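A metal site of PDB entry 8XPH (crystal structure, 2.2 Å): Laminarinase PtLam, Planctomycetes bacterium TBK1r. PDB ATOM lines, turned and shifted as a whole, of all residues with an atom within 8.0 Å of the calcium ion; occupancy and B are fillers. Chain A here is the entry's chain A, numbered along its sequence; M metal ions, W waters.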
ATOM      1  N   PRO A 117      25.679 -19.527 -24.870  1.00  0.00           N
ATOM      2  CA  PRO A 117      25.184 -20.702 -25.591  1.00  0.00           C
ATOM      3  C   PRO A 117      25.625 -22.086 -25.104  1.00  0.00           C
ATOM      4  O   PRO A 117      25.614 -23.036 -25.885  1.00  0.00           O
ATOM      5  CB  PRO A 117      25.802 -20.388 -26.970  1.00  0.00           C
ATOM      6  CG  PRO A 117      27.186 -19.882 -26.645  1.00  0.00           C
ATOM      7  CD  PRO A 117      26.992 -19.078 -25.373  1.00  0.00           C
ATOM      8  N   LYS A 118      25.969 -22.209 -23.812  1.00  0.00           N
ATOM      9  CA  LYS A 118      26.393 -23.487 -23.267  1.00  0.00           C
ATOM     10  C   LYS A 118      25.218 -24.466 -23.201  1.00  0.00           C
ATOM     11  O   LYS A 118      25.408 -25.679 -23.168  1.00  0.00           O
ATOM     12  CB  LYS A 118      27.016 -23.310 -21.878  1.00  0.00           C
ATOM     13  CG  LYS A 118      28.362 -22.614 -21.870  1.00  0.00           C
ATOM     14  CD  LYS A 118      28.751 -22.027 -20.522  1.00  0.00           C
ATOM     15  CE  LYS A 118      30.011 -21.203 -20.610  1.00  0.00           C
ATOM     16  NZ  LYS A 118      30.383 -20.646 -19.309  1.00  0.00           N
ATOM     17  N   CYS A 119      23.991 -23.922 -23.153  1.00  0.00           N
ATOM     18  CA  CYS A 119      22.768 -24.711 -23.219  1.00  0.00           C
ATOM     19  C   CYS A 119      22.625 -25.365 -24.588  1.00  0.00           C
ATOM     20  O   CYS A 119      22.024 -26.430 -24.698  1.00  0.00           O
ATOM     21  CB  CYS A 119      21.555 -23.830 -22.956  1.00  0.00           C
ATOM     22  SG  CYS A 119      21.403 -22.473 -24.146  1.00  0.00           S
ATOM     23  N   GLY A 120      23.149 -24.711 -25.626  1.00  0.00           N
ATOM     24  CA  GLY A 120      23.036 -25.210 -26.986  1.00  0.00           C
ATOM     25  C   GLY A 120      21.781 -24.654 -27.660  1.00  0.00           C
ATOM     26  O   GLY A 120      20.805 -24.311 -26.983  1.00  0.00           O
ATOM     27  N   PHE A 148      26.505 -22.804 -29.941  1.00  0.00           N
ATOM     28  CA  PHE A 148      26.946 -23.586 -28.794  1.00  0.00           C
ATOM     29  C   PHE A 148      28.272 -23.055 -28.281  1.00  0.00           C
ATOM     30  O   PHE A 148      28.840 -22.125 -28.861  1.00  0.00           O
ATOM     31  CB  PHE A 148      27.042 -25.058 -29.194  1.00  0.00           C
ATOM     32  CG  PHE A 148      27.987 -25.348 -30.363  1.00  0.00           C
ATOM     33  CD1 PHE A 148      27.605 -25.083 -31.666  1.00  0.00           C
ATOM     34  CD2 PHE A 148      29.241 -25.915 -30.144  1.00  0.00           C
ATOM     35  CE1 PHE A 148      28.457 -25.342 -32.726  1.00  0.00           C
ATOM     36  CE2 PHE A 148      30.085 -26.180 -31.203  1.00  0.00           C
ATOM     37  CZ  PHE A 148      29.702 -25.896 -32.494  1.00  0.00           C
ATOM     38  N   ALA A 149      28.746 -23.642 -27.179  1.00  0.00           N
ATOM     39  CA  ALA A 149      30.088 -23.384 -26.667  1.00  0.00           C
ATOM     40  C   ALA A 149      31.065 -24.388 -27.269  1.00  0.00           C
ATOM     41  O   ALA A 149      31.012 -25.580 -26.974  1.00  0.00           O
ATOM     42  CB  ALA A 149      30.080 -23.451 -25.148  1.00  0.00           C
ATOM     43  N   GLY A 150      31.954 -23.898 -28.144  1.00  0.00           N
ATOM     44  CA  GLY A 150      32.858 -24.763 -28.893  1.00  0.00           C
ATOM     45  C   GLY A 150      34.081 -25.139 -28.070  1.00  0.00           C
ATOM     46  O   GLY A 150      34.026 -25.176 -26.841  1.00  0.00           O
ATOM     47  N   VAL A 151      35.188 -25.423 -28.773  1.00  0.00           N
ATOM     48  CA  VAL A 151      36.465 -25.661 -28.130  1.00  0.00           C
ATOM     49  C   VAL A 151      36.741 -24.498 -27.192  1.00  0.00           C
ATOM     50  O   VAL A 151      36.556 -23.339 -27.567  1.00  0.00           O
ATOM     51  CB  VAL A 151      37.593 -25.829 -29.174  1.00  0.00           C
ATOM     52  CG1 VAL A 151      38.984 -25.703 -28.574  1.00  0.00           C
ATOM     53  CG2 VAL A 151      37.457 -27.147 -29.934  1.00  0.00           C
ATOM     54  N   GLY A 152      37.139 -24.806 -25.962  1.00  0.00           N
ATOM     55  CA  GLY A 152      37.475 -23.791 -24.989  1.00  0.00           C
ATOM     56  C   GLY A 152      36.240 -23.065 -24.458  1.00  0.00           C
ATOM     57  O   GLY A 152      36.377 -22.028 -23.799  1.00  0.00           O
ATOM     58  N   GLU A 153      35.047 -23.609 -24.731  1.00  0.00           N
ATOM     59  CA  GLU A 153      33.807 -23.169 -24.108  1.00  0.00           C
ATOM     60  C   GLU A 153      33.418 -21.770 -24.589  1.00  0.00           C
ATOM     61  O   GLU A 153      32.753 -21.026 -23.862  1.00  0.00           O
ATOM     62  CB  GLU A 153      33.915 -23.187 -22.586  1.00  0.00           C
ATOM     63  CG  GLU A 153      34.388 -24.523 -22.011  1.00  0.00           C
ATOM     64  CD  GLU A 153      33.521 -25.701 -22.412  1.00  0.00           C
ATOM     65  OE1 GLU A 153      32.302 -25.592 -22.161  1.00  0.00           O
ATOM     66  OE2 GLU A 153      34.038 -26.691 -22.969  1.00  0.00           O
ATOM     67  N   GLN A 154      33.794 -21.413 -25.822  1.00  0.00           N
ATOM     68  CA  GLN A 154      33.513 -20.087 -26.342  1.00  0.00           C
ATOM     69  C   GLN A 154      32.483 -20.182 -27.458  1.00  0.00           C
ATOM     70  O   GLN A 154      32.446 -21.172 -28.170  1.00  0.00           O
ATOM     71  CB  GLN A 154      34.779 -19.389 -26.841  1.00  0.00           C
ATOM     72  CG  GLN A 154      35.785 -19.075 -25.738  1.00  0.00           C
ATOM     73  CD  GLN A 154      35.241 -18.205 -24.632  1.00  0.00           C
ATOM     74  OE1 GLN A 154      34.719 -17.111 -24.872  1.00  0.00           O
ATOM     75  NE2 GLN A 154      35.336 -18.680 -23.396  1.00  0.00           N
ATOM     76  N   THR A 156      30.380 -20.464 -30.528  1.00  0.00           N
ATOM     77  CA  THR A 156      30.652 -20.913 -31.891  1.00  0.00           C
ATOM     78  C   THR A 156      29.335 -20.955 -32.650  1.00  0.00           C
ATOM     79  O   THR A 156      28.311 -21.342 -32.091  1.00  0.00           O
ATOM     80  CB  THR A 156      31.336 -22.275 -31.886  1.00  0.00           C
ATOM     81  OG1 THR A 156      32.544 -22.088 -31.162  1.00  0.00           O
ATOM     82  CG2 THR A 156      31.638 -22.796 -33.283  1.00  0.00           C
ATOM     83  N   ALA A 200      31.596 -34.682 -31.851  1.00  0.00           N
ATOM     84  CA  ALA A 200      32.841 -34.101 -31.353  1.00  0.00           C
ATOM     85  C   ALA A 200      32.687 -33.660 -29.893  1.00  0.00           C
ATOM     86  O   ALA A 200      31.592 -33.320 -29.446  1.00  0.00           O
ATOM     87  CB  ALA A 200      33.255 -32.932 -32.222  1.00  0.00           C
ATOM     88  N   SER A 201      33.818 -33.650 -29.191  1.00  0.00           N
ATOM     89  CA  SER A 201      33.873 -33.484 -27.750  1.00  0.00           C
ATOM     90  C   SER A 201      33.240 -32.171 -27.299  1.00  0.00           C
ATOM     91  O   SER A 201      32.723 -32.080 -26.189  1.00  0.00           O
ATOM     92  CB  SER A 201      35.290 -33.589 -27.249  1.00  0.00           C
ATOM     93  OG  SER A 201      36.083 -32.520 -27.769  1.00  0.00           O
ATOM     94  N   GLU A 202      33.292 -31.143 -28.152  1.00  0.00           N
ATOM     95  CA  GLU A 202      32.822 -29.816 -27.770  1.00  0.00           C
ATOM     96  C   GLU A 202      31.324 -29.651 -28.038  1.00  0.00           C
ATOM     97  O   GLU A 202      30.797 -28.569 -27.806  1.00  0.00           O
ATOM     98  CB  GLU A 202      33.640 -28.712 -28.451  1.00  0.00           C
ATOM     99  CG  GLU A 202      33.499 -28.619 -29.963  1.00  0.00           C
ATOM    100  CD  GLU A 202      34.390 -29.524 -30.793  1.00  0.00           C
ATOM    101  OE1 GLU A 202      35.067 -30.395 -30.214  1.00  0.00           O
ATOM    102  OE2 GLU A 202      34.422 -29.333 -32.034  1.00  0.00           O
ATOM    103  N   MET A 203      30.646 -30.717 -28.478  1.00  0.00           N
ATOM    104  CA  MET A 203      29.240 -30.614 -28.872  1.00  0.00           C
ATOM    105  C   MET A 203      28.374 -31.549 -28.027  1.00  0.00           C
ATOM    106  O   MET A 203      27.347 -32.031 -28.497  1.00  0.00           O
ATOM    107  CB  MET A 203      29.076 -30.953 -30.366  1.00  0.00           C
ATOM    108  CG  MET A 203      29.935 -30.097 -31.279  1.00  0.00           C
ATOM    109  SD  MET A 203      29.663 -30.422 -33.026  1.00  0.00           S
ATOM    110  CE  MET A 203      28.095 -29.622 -33.346  1.00  0.00           C
ATOM    111  N   LYS A 204      28.778 -31.766 -26.773  1.00  0.00           N
ATOM    112  CA  LYS A 204      28.038 -32.626 -25.864  1.00  0.00           C
ATOM    113  C   LYS A 204      26.727 -31.958 -25.427  1.00  0.00           C
ATOM    114  O   LYS A 204      25.840 -32.645 -24.913  1.00  0.00           O
ATOM    115  CB  LYS A 204      28.884 -33.009 -24.643  1.00  0.00           C
ATOM    116  CG  LYS A 204      29.973 -34.039 -24.911  1.00  0.00           C
ATOM    117  CD  LYS A 204      30.556 -34.650 -23.640  1.00  0.00           C
ATOM    118  CE  LYS A 204      31.673 -35.617 -23.887  1.00  0.00           C
ATOM    119  NZ  LYS A 204      32.924 -34.950 -24.255  1.00  0.00           N
ATOM    120  N   GLU A 205      26.598 -30.647 -25.642  1.00  0.00           N
ATOM    121  CA  GLU A 205      25.375 -29.923 -25.324  1.00  0.00           C
ATOM    122  C   GLU A 205      24.207 -30.426 -26.165  1.00  0.00           C
ATOM    123  O   GLU A 205      23.054 -30.167 -25.824  1.00  0.00           O
ATOM    124  CB  GLU A 205      25.393 -28.418 -25.609  1.00  0.00           C
ATOM    125  CG  GLU A 205      26.575 -27.670 -25.005  1.00  0.00           C
ATOM    126  CD  GLU A 205      27.798 -27.592 -25.907  1.00  0.00           C
ATOM    127  OE1 GLU A 205      28.346 -28.663 -26.247  1.00  0.00           O
ATOM    128  OE2 GLU A 205      28.192 -26.459 -26.259  1.00  0.00           O
ATOM    129  N   TYR A 206      24.505 -31.104 -27.279  1.00  0.00           N
ATOM    130  CA  TYR A 206      23.484 -31.527 -28.219  1.00  0.00           C
ATOM    131  C   TYR A 206      23.057 -32.977 -27.957  1.00  0.00           C
ATOM    132  O   TYR A 206      22.412 -33.585 -28.815  1.00  0.00           O
ATOM    133  CB  TYR A 206      24.001 -31.331 -29.650  1.00  0.00           C
ATOM    134  CG  TYR A 206      24.098 -29.872 -30.070  1.00  0.00           C
ATOM    135  CD1 TYR A 206      22.955 -29.101 -30.205  1.00  0.00           C
ATOM    136  CD2 TYR A 206      25.331 -29.271 -30.337  1.00  0.00           C
ATOM    137  CE1 TYR A 206      23.028 -27.768 -30.596  1.00  0.00           C
ATOM    138  CE2 TYR A 206      25.417 -27.953 -30.719  1.00  0.00           C
ATOM    139  CZ  TYR A 206      24.267 -27.188 -30.854  1.00  0.00           C
ATOM    140  OH  TYR A 206      24.330 -25.890 -31.234  1.00  0.00           O
HETATM  141 CA    CA M   1      30.393 -27.438 -25.817  1.00  0.00          CA
HETATM  142  O   HOH W   1      31.090 -29.943 -24.972  1.00  0.00           O
HETATM  143  O   HOH W   2      30.092 -26.979 -23.558  1.00  0.00           O
HETATM  144  O   HOH W   3      32.674 -27.093 -25.274  1.00  0.00           O
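Of the 19 residues printed, 3 come within 4 Å of the calcium ion.
The calcium ion is bound by O of Ala 149 (2.3 Å), O of Glu 202 (2.3 Å), water W2 (2.3 Å), water W3 (2.4 Å), OE1 of Glu 205 (2.4 Å), OE2 of Glu 205 (2.4 Å) and water W1 (2.7 Å).
The backbone carbonyl oxygen of Pro 117 is in hydrogen-bond range of the backbone NH of Ala 149, at 3.4 Å.
OG of Ser 201 sits at hydrogen-bond distance from OE1 of Glu 202 (3.4 Å).
Water W3 bridges OE2 of Glu 153 and O of Gly 150.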
